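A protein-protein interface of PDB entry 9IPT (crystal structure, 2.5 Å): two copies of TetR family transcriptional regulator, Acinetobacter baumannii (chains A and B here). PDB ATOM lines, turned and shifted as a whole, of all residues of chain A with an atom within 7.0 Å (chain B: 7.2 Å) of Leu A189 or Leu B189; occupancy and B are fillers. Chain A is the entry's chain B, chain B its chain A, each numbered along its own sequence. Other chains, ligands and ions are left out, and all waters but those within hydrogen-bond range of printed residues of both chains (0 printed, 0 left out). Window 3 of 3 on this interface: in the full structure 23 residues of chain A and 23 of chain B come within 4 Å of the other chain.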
ATOM      1  N   ARG A 146      -7.094  20.631 -22.895  1.00  0.00           N
ATOM      2  CA  ARG A 146      -7.964  20.058 -21.873  1.00  0.00           C
ATOM      3  C   ARG A 146      -9.358  20.673 -21.915  1.00  0.00           C
ATOM      4  O   ARG A 146     -10.361  19.957 -21.811  1.00  0.00           O
ATOM      5  CB  ARG A 146      -7.341  20.242 -20.490  1.00  0.00           C
ATOM      6  CG  ARG A 146      -6.761  18.969 -19.897  1.00  0.00           C
ATOM      7  CD  ARG A 146      -5.657  19.278 -18.901  1.00  0.00           C
ATOM      8  NE  ARG A 146      -4.330  19.123 -19.483  1.00  0.00           N
ATOM      9  CZ  ARG A 146      -3.220  18.957 -18.778  1.00  0.00           C
ATOM     10  NH1 ARG A 146      -3.239  18.928 -17.456  1.00  0.00           N
ATOM     11  NH2 ARG A 146      -2.061  18.817 -19.415  1.00  0.00           N
ATOM     12  N   ARG A 155     -11.181  31.535 -16.008  1.00  0.00           N
ATOM     13  CA  ARG A 155     -10.694  30.963 -14.758  1.00  0.00           C
ATOM     14  C   ARG A 155      -9.366  31.586 -14.346  1.00  0.00           C
ATOM     15  O   ARG A 155      -9.111  31.784 -13.152  1.00  0.00           O
ATOM     16  CB  ARG A 155     -10.555  29.448 -14.894  1.00  0.00           C
ATOM     17  CG  ARG A 155     -11.803  28.675 -14.509  1.00  0.00           C
ATOM     18  CD  ARG A 155     -11.583  27.177 -14.637  1.00  0.00           C
ATOM     19  NE  ARG A 155     -12.553  26.560 -15.532  1.00  0.00           N
ATOM     20  CZ  ARG A 155     -12.243  25.712 -16.504  1.00  0.00           C
ATOM     21  NH1 ARG A 155     -10.991  25.354 -16.733  1.00  0.00           N
ATOM     22  NH2 ARG A 155     -13.214  25.213 -17.263  1.00  0.00           N
ATOM     23  N   HIS A 182       1.836  30.822  -7.034  1.00  0.00           N
ATOM     24  CA  HIS A 182       0.481  30.299  -7.196  1.00  0.00           C
ATOM     25  C   HIS A 182      -0.019  30.489  -8.621  1.00  0.00           C
ATOM     26  O   HIS A 182      -0.713  29.618  -9.161  1.00  0.00           O
ATOM     27  CB  HIS A 182      -0.466  30.967  -6.203  1.00  0.00           C
ATOM     28  CG  HIS A 182      -0.230  30.568  -4.781  1.00  0.00           C
ATOM     29  ND1 HIS A 182      -0.376  29.271  -4.337  1.00  0.00           N
ATOM     30  CD2 HIS A 182       0.131  31.297  -3.698  1.00  0.00           C
ATOM     31  CE1 HIS A 182      -0.107  29.217  -3.046  1.00  0.00           C
ATOM     32  NE2 HIS A 182       0.204  30.433  -2.633  1.00  0.00           N
ATOM     33  N   GLU A 184       1.931  30.600 -11.312  1.00  0.00           N
ATOM     34  CA  GLU A 184       2.658  29.611 -12.102  1.00  0.00           C
ATOM     35  C   GLU A 184       2.020  28.235 -11.983  1.00  0.00           C
ATOM     36  O   GLU A 184       1.971  27.477 -12.959  1.00  0.00           O
ATOM     37  CB  GLU A 184       4.122  29.553 -11.665  1.00  0.00           C
ATOM     38  CG  GLU A 184       5.056  28.986 -12.722  1.00  0.00           C
ATOM     39  CD  GLU A 184       6.205  28.196 -12.129  1.00  0.00           C
ATOM     40  OE1 GLU A 184       7.157  28.822 -11.619  1.00  0.00           O
ATOM     41  OE2 GLU A 184       6.156  26.948 -12.176  1.00  0.00           O
ATOM     42  N   ALA A 185       1.525  27.898 -10.791  1.00  0.00           N
ATOM     43  CA  ALA A 185       0.860  26.616 -10.595  1.00  0.00           C
ATOM     44  C   ALA A 185      -0.394  26.519 -11.455  1.00  0.00           C
ATOM     45  O   ALA A 185      -0.496  25.651 -12.328  1.00  0.00           O
ATOM     46  CB  ALA A 185       0.523  26.423  -9.115  1.00  0.00           C
ATOM     47  N   ILE A 186      -1.346  27.433 -11.237  1.00  0.00           N
ATOM     48  CA  ILE A 186      -2.651  27.361 -11.896  1.00  0.00           C
ATOM     49  C   ILE A 186      -2.500  27.279 -13.411  1.00  0.00           C
ATOM     50  O   ILE A 186      -3.273  26.592 -14.090  1.00  0.00           O
ATOM     51  CB  ILE A 186      -3.520  28.563 -11.476  1.00  0.00           C
ATOM     52  CG1 ILE A 186      -3.764  28.532  -9.968  1.00  0.00           C
ATOM     53  CG2 ILE A 186      -4.843  28.565 -12.223  1.00  0.00           C
ATOM     54  CD1 ILE A 186      -4.621  27.371  -9.515  1.00  0.00           C
ATOM     55  N   ILE A 187      -1.498  27.967 -13.965  1.00  0.00           N
ATOM     56  CA  ILE A 187      -1.249  27.873 -15.401  1.00  0.00           C
ATOM     57  C   ILE A 187      -0.840  26.455 -15.779  1.00  0.00           C
ATOM     58  O   ILE A 187      -1.238  25.936 -16.829  1.00  0.00           O
ATOM     59  CB  ILE A 187      -0.187  28.903 -15.832  1.00  0.00           C
ATOM     60  CG1 ILE A 187      -0.661  30.325 -15.532  1.00  0.00           C
ATOM     61  CG2 ILE A 187       0.127  28.760 -17.313  1.00  0.00           C
ATOM     62  CD1 ILE A 187       0.434  31.366 -15.646  1.00  0.00           C
ATOM     63  N   ARG A 188      -0.050  25.799 -14.923  1.00  0.00           N
ATOM     64  CA  ARG A 188       0.417  24.451 -15.235  1.00  0.00           C
ATOM     65  C   ARG A 188      -0.725  23.440 -15.202  1.00  0.00           C
ATOM     66  O   ARG A 188      -0.811  22.572 -16.079  1.00  0.00           O
ATOM     67  CB  ARG A 188       1.528  24.043 -14.269  1.00  0.00           C
ATOM     68  CG  ARG A 188       2.864  24.721 -14.537  1.00  0.00           C
ATOM     69  CD  ARG A 188       3.915  24.293 -13.520  1.00  0.00           C
ATOM     70  NE  ARG A 188       5.155  25.053 -13.640  1.00  0.00           N
ATOM     71  CZ  ARG A 188       5.987  24.988 -14.671  1.00  0.00           C
ATOM     72  NH1 ARG A 188       5.759  24.184 -15.696  1.00  0.00           N
ATOM     73  NH2 ARG A 188       7.080  25.747 -14.670  1.00  0.00           N
ATOM     74  N   LEU A 189      -1.607  23.526 -14.202  1.00  0.00           N
ATOM     75  CA  LEU A 189      -2.733  22.598 -14.146  1.00  0.00           C
ATOM     76  C   LEU A 189      -3.689  22.791 -15.317  1.00  0.00           C
ATOM     77  O   LEU A 189      -4.343  21.833 -15.744  1.00  0.00           O
ATOM     78  CB  LEU A 189      -3.503  22.741 -12.829  1.00  0.00           C
ATOM     79  CG  LEU A 189      -2.894  22.360 -11.473  1.00  0.00           C
ATOM     80  CD1 LEU A 189      -2.287  20.961 -11.526  1.00  0.00           C
ATOM     81  CD2 LEU A 189      -1.897  23.377 -10.946  1.00  0.00           C
ATOM     82  N   GLU A 190      -3.784  24.009 -15.847  1.00  0.00           N
ATOM     83  CA  GLU A 190      -4.784  24.316 -16.862  1.00  0.00           C
ATOM     84  C   GLU A 190      -4.322  23.963 -18.273  1.00  0.00           C
ATOM     85  O   GLU A 190      -5.075  23.352 -19.038  1.00  0.00           O
ATOM     86  CB  GLU A 190      -5.163  25.798 -16.792  1.00  0.00           C
ATOM     87  CG  GLU A 190      -6.130  26.141 -15.668  1.00  0.00           C
ATOM     88  CD  GLU A 190      -7.576  25.876 -16.042  1.00  0.00           C
ATOM     89  OE1 GLU A 190      -7.831  25.502 -17.205  1.00  0.00           O
ATOM     90  OE2 GLU A 190      -8.457  26.046 -15.173  1.00  0.00           O
ATOM     91  N   LEU A 191      -3.098  24.337 -18.637  1.00  0.00           N
ATOM     92  CA  LEU A 191      -2.634  24.195 -20.013  1.00  0.00           C
ATOM     93  C   LEU A 191      -1.383  23.348 -20.160  1.00  0.00           C
ATOM     94  O   LEU A 191      -1.263  22.607 -21.139  1.00  0.00           O
ATOM     95  CB  LEU A 191      -2.379  25.578 -20.627  1.00  0.00           C
ATOM     96  CG  LEU A 191      -3.532  26.576 -20.533  1.00  0.00           C
ATOM     97  CD1 LEU A 191      -3.015  27.964 -20.200  1.00  0.00           C
ATOM     98  CD2 LEU A 191      -4.321  26.588 -21.828  1.00  0.00           C
ATOM     99  N   LEU A 192      -0.441  23.441 -19.229  1.00  0.00           N
ATOM    100  CA  LEU A 192       0.815  22.708 -19.347  1.00  0.00           C
ATOM    101  C   LEU A 192       0.695  21.297 -18.783  1.00  0.00           C
ATOM    102  O   LEU A 192      -0.303  20.607 -18.995  1.00  0.00           O
ATOM    103  CB  LEU A 192       1.944  23.462 -18.640  1.00  0.00           C
ATOM    104  CG  LEU A 192       3.254  23.601 -19.418  1.00  0.00           C
ATOM    105  CD1 LEU A 192       2.982  23.819 -20.900  1.00  0.00           C
ATOM    106  CD2 LEU A 192       4.093  24.736 -18.851  1.00  0.00           C
ATOM    107  OXT LEU A 192       1.600  20.809 -18.106  1.00  0.00           O
ATOM    108  N   ARG B 146      -0.879  16.135  -5.246  1.00  0.00           N
ATOM    109  CA  ARG B 146      -0.103  16.857  -6.247  1.00  0.00           C
ATOM    110  C   ARG B 146       0.710  18.003  -5.657  1.00  0.00           C
ATOM    111  O   ARG B 146       1.781  18.324  -6.186  1.00  0.00           O
ATOM    112  CB  ARG B 146      -1.028  17.388  -7.346  1.00  0.00           C
ATOM    113  CG  ARG B 146      -1.397  16.352  -8.394  1.00  0.00           C
ATOM    114  CD  ARG B 146      -2.273  16.943  -9.485  1.00  0.00           C
ATOM    115  NE  ARG B 146      -3.411  16.082  -9.787  1.00  0.00           N
ATOM    116  CZ  ARG B 146      -3.432  15.191 -10.768  1.00  0.00           C
ATOM    117  NH1 ARG B 146      -2.393  15.018 -11.569  1.00  0.00           N
ATOM    118  NH2 ARG B 146      -4.522  14.451 -10.949  1.00  0.00           N
ATOM    119  N   SER B 147       0.238  18.631  -4.581  1.00  0.00           N
ATOM    120  CA  SER B 147       0.901  19.817  -4.058  1.00  0.00           C
ATOM    121  C   SER B 147       0.624  19.955  -2.565  1.00  0.00           C
ATOM    122  O   SER B 147      -0.044  19.119  -1.951  1.00  0.00           O
ATOM    123  CB  SER B 147       0.453  21.069  -4.819  1.00  0.00           C
ATOM    124  OG  SER B 147       1.223  22.196  -4.445  1.00  0.00           O
ATOM    125  N   ILE B 152      -3.068  24.364  -1.753  1.00  0.00           N
ATOM    126  CA  ILE B 152      -4.322  24.069  -2.442  1.00  0.00           C
ATOM    127  C   ILE B 152      -5.463  24.864  -1.824  1.00  0.00           C
ATOM    128  O   ILE B 152      -6.302  25.430  -2.533  1.00  0.00           O
ATOM    129  CB  ILE B 152      -4.626  22.557  -2.416  1.00  0.00           C
ATOM    130  CG1 ILE B 152      -3.369  21.730  -2.684  1.00  0.00           C
ATOM    131  CG2 ILE B 152      -5.718  22.219  -3.423  1.00  0.00           C
ATOM    132  CD1 ILE B 152      -3.068  21.520  -4.142  1.00  0.00           C
ATOM    133  N   ARG B 155      -5.384  28.601  -2.826  1.00  0.00           N
ATOM    134  CA  ARG B 155      -5.768  28.793  -4.221  1.00  0.00           C
ATOM    135  C   ARG B 155      -7.248  28.498  -4.429  1.00  0.00           C
ATOM    136  O   ARG B 155      -7.907  29.149  -5.249  1.00  0.00           O
ATOM    137  CB  ARG B 155      -4.910  27.915  -5.130  1.00  0.00           C
ATOM    138  CG  ARG B 155      -3.440  28.299  -5.145  1.00  0.00           C
ATOM    139  CD  ARG B 155      -2.713  27.674  -6.323  1.00  0.00           C
ATOM    140  NE  ARG B 155      -2.746  26.218  -6.273  1.00  0.00           N
ATOM    141  CZ  ARG B 155      -1.753  25.459  -5.830  1.00  0.00           C
ATOM    142  NH1 ARG B 155      -0.628  25.988  -5.378  1.00  0.00           N
ATOM    143  NH2 ARG B 155      -1.890  24.137  -5.844  1.00  0.00           N
ATOM    144  N   GLU B 184     -16.032  23.238 -10.099  1.00  0.00           N
ATOM    145  CA  GLU B 184     -15.819  21.802 -10.233  1.00  0.00           C
ATOM    146  C   GLU B 184     -14.529  21.507 -10.988  1.00  0.00           C
ATOM    147  O   GLU B 184     -13.731  20.657 -10.573  1.00  0.00           O
ATOM    148  CB  GLU B 184     -17.011  21.164 -10.947  1.00  0.00           C
ATOM    149  CG  GLU B 184     -17.537  19.899 -10.299  1.00  0.00           C
ATOM    150  CD  GLU B 184     -18.867  19.465 -10.881  1.00  0.00           C
ATOM    151  OE1 GLU B 184     -19.872  19.469 -10.140  1.00  0.00           O
ATOM    152  OE2 GLU B 184     -18.909  19.125 -12.083  1.00  0.00           O
ATOM    153  N   ALA B 185     -14.304  22.210 -12.102  1.00  0.00           N
ATOM    154  CA  ALA B 185     -13.147  21.925 -12.944  1.00  0.00           C
ATOM    155  C   ALA B 185     -11.840  22.236 -12.225  1.00  0.00           C
ATOM    156  O   ALA B 185     -10.845  21.522 -12.395  1.00  0.00           O
ATOM    157  CB  ALA B 185     -13.244  22.718 -14.248  1.00  0.00           C
ATOM    158  N   ILE B 186     -11.824  23.296 -11.414  1.00  0.00           N
ATOM    159  CA  ILE B 186     -10.598  23.678 -10.720  1.00  0.00           C
ATOM    160  C   ILE B 186     -10.260  22.666  -9.632  1.00  0.00           C
ATOM    161  O   ILE B 186      -9.084  22.362  -9.391  1.00  0.00           O
ATOM    162  CB  ILE B 186     -10.732  25.108 -10.163  1.00  0.00           C
ATOM    163  CG1 ILE B 186     -10.385  26.130 -11.247  1.00  0.00           C
ATOM    164  CG2 ILE B 186      -9.849  25.311  -8.937  1.00  0.00           C
ATOM    165  CD1 ILE B 186      -8.923  26.125 -11.641  1.00  0.00           C
ATOM    166  N   ILE B 187     -11.279  22.115  -8.969  1.00  0.00           N
ATOM    167  CA  ILE B 187     -11.032  21.114  -7.937  1.00  0.00           C
ATOM    168  C   ILE B 187     -10.450  19.846  -8.551  1.00  0.00           C
ATOM    169  O   ILE B 187      -9.521  19.243  -8.001  1.00  0.00           O
ATOM    170  CB  ILE B 187     -12.324  20.820  -7.153  1.00  0.00           C
ATOM    171  CG1 ILE B 187     -12.713  22.018  -6.290  1.00  0.00           C
ATOM    172  CG2 ILE B 187     -12.147  19.594  -6.273  1.00  0.00           C
ATOM    173  CD1 ILE B 187     -14.006  21.822  -5.529  1.00  0.00           C
ATOM    174  N   ARG B 188     -10.985  19.423  -9.700  1.00  0.00           N
ATOM    175  CA  ARG B 188     -10.485  18.215 -10.349  1.00  0.00           C
ATOM    176  C   ARG B 188      -9.027  18.370 -10.761  1.00  0.00           C
ATOM    177  O   ARG B 188      -8.233  17.434 -10.621  1.00  0.00           O
ATOM    178  CB  ARG B 188     -11.350  17.872 -11.561  1.00  0.00           C
ATOM    179  CG  ARG B 188     -12.610  17.091 -11.227  1.00  0.00           C
ATOM    180  CD  ARG B 188     -13.697  17.332 -12.265  1.00  0.00           C
ATOM    181  NE  ARG B 188     -14.933  16.625 -11.950  1.00  0.00           N
ATOM    182  CZ  ARG B 188     -15.092  15.310 -12.026  1.00  0.00           C
ATOM    183  NH1 ARG B 188     -14.112  14.517 -12.426  1.00  0.00           N
ATOM    184  NH2 ARG B 188     -16.267  14.778 -11.699  1.00  0.00           N
ATOM    185  N   LEU B 189      -8.655  19.547 -11.268  1.00  0.00           N
ATOM    186  CA  LEU B 189      -7.271  19.771 -11.672  1.00  0.00           C
ATOM    187  C   LEU B 189      -6.332  19.807 -10.473  1.00  0.00           C
ATOM    188  O   LEU B 189      -5.158  19.437 -10.596  1.00  0.00           O
ATOM    189  CB  LEU B 189      -7.157  21.072 -12.466  1.00  0.00           C
ATOM    190  CG  LEU B 189      -7.115  20.974 -13.992  1.00  0.00           C
ATOM    191  CD1 LEU B 189      -8.116  19.952 -14.511  1.00  0.00           C
ATOM    192  CD2 LEU B 189      -7.367  22.339 -14.615  1.00  0.00           C
ATOM    193  N   GLU B 190      -6.827  20.239  -9.315  1.00  0.00           N
ATOM    194  CA  GLU B 190      -5.980  20.398  -8.140  1.00  0.00           C
ATOM    195  C   GLU B 190      -5.859  19.117  -7.323  1.00  0.00           C
ATOM    196  O   GLU B 190      -4.764  18.785  -6.857  1.00  0.00           O
ATOM    197  CB  GLU B 190      -6.521  21.522  -7.251  1.00  0.00           C
ATOM    198  CG  GLU B 190      -6.115  22.931  -7.675  1.00  0.00           C
ATOM    199  CD  GLU B 190      -4.709  23.305  -7.242  1.00  0.00           C
ATOM    200  OE1 GLU B 190      -3.878  22.398  -7.021  1.00  0.00           O
ATOM    201  OE2 GLU B 190      -4.433  24.517  -7.115  1.00  0.00           O
ATOM    202  N   LEU B 191      -6.961  18.387  -7.137  1.00  0.00           N
ATOM    203  CA  LEU B 191      -6.974  17.234  -6.249  1.00  0.00           C
ATOM    204  C   LEU B 191      -7.326  15.917  -6.923  1.00  0.00           C
ATOM    205  O   LEU B 191      -6.966  14.863  -6.388  1.00  0.00           O
ATOM    206  CB  LEU B 191      -7.958  17.466  -5.091  1.00  0.00           C
ATOM    207  CG  LEU B 191      -7.614  18.633  -4.165  1.00  0.00           C
ATOM    208  CD1 LEU B 191      -8.864  19.162  -3.484  1.00  0.00           C
ATOM    209  CD2 LEU B 191      -6.573  18.214  -3.140  1.00  0.00           C
ATOM    210  N   LEU B 192      -8.013  15.937  -8.061  1.00  0.00           N
ATOM    211  CA  LEU B 192      -8.377  14.700  -8.745  1.00  0.00           C
ATOM    212  C   LEU B 192      -7.484  14.460  -9.959  1.00  0.00           C
ATOM    213  O   LEU B 192      -7.653  13.485 -10.690  1.00  0.00           O
ATOM    214  CB  LEU B 192      -9.847  14.729  -9.171  1.00  0.00           C
ATOM    215  CG  LEU B 192     -10.895  14.686  -8.054  1.00  0.00           C
ATOM    216  CD1 LEU B 192     -12.214  14.139  -8.579  1.00  0.00           C
ATOM    217  CD2 LEU B 192     -10.403  13.855  -6.880  1.00  0.00           C
ATOM    218  OXT LEU B 192      -6.569  15.236 -10.236  1.00  0.00           O
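NH1 of Arg B155 sits close to ND1 of His A182 (3.5 Å).
The guanidinium group (NE) of Arg B155 lies within salt-bridge range of the side-chain carboxylate (OE2) of Glu B190. OE2 of Glu A190 is in salt-bridge range of NH1 of Arg A155.
Among the printed residues, merely in contact across the chains: Leu A189 with Leu B189, Glu A190 with Ile B186, Ile A186 with Arg B155, Ile A186 with Glu B190, Arg A155 with Ile B186, Glu A190 with Leu B189, Arg A155 with Ala B185 and Ala A185 with Arg B155.
Leu A189 touches just one residue of chain B: Leu B189 (3.3 Å). Of chain A, only Leu A189 (3.3 Å) and Glu A190 (3.8 Å) come within 4 Å of Leu B189. Of the printed residues of chain A, Ile B186 touches Arg A155 (3.7 Å) and Glu A190 (3.6 Å). Of the printed residues of chain B, Glu A190 touches Ile B186 and Leu B189. Of the printed residues of chain B, Arg A155 touches Ala B185 (3.9 Å) and Ile B186 (3.7 Å). Leu B191 touches none of the printed residues of chain A.
Of the 12 printed residues of chain A, 6 touch a printed residue of chain B. Hydrophobic or aromatic side chains of chain A within 4 Å of the printed part of chain B: His A182, Ala A185, Ile A186 and Leu A189. Along chain A the printed residues that touch a printed residue of chain B span positions 155 to 190. Hydrophobic or aromatic side chains of chain B within 4 Å of the printed part of chain A: Ala B185, Ile B186 and Leu B189. Among the printed residues, 9 pairs touch across the chains. Among the printed residues, no Asp or Glu carboxylate lies within 4 Å of a Lys or Arg side-chain nitrogen of the other chain.
Arg A155 touches Ile B186, and with the chains exchanged Ile A186 touches Arg B155. Ile A186 touches Glu B190, and with the chains exchanged Glu A190 touches Ile B186. Leu A189 touches its own counterpart, Leu B189. Glu A190 touches Leu B189, but with the chains exchanged Leu A189 does not touch Glu B190 (4.5 Å). Positions printed for both chains: 146, 155, 184, 185, 186, 187, 188, 189, 190, 191 and 192.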
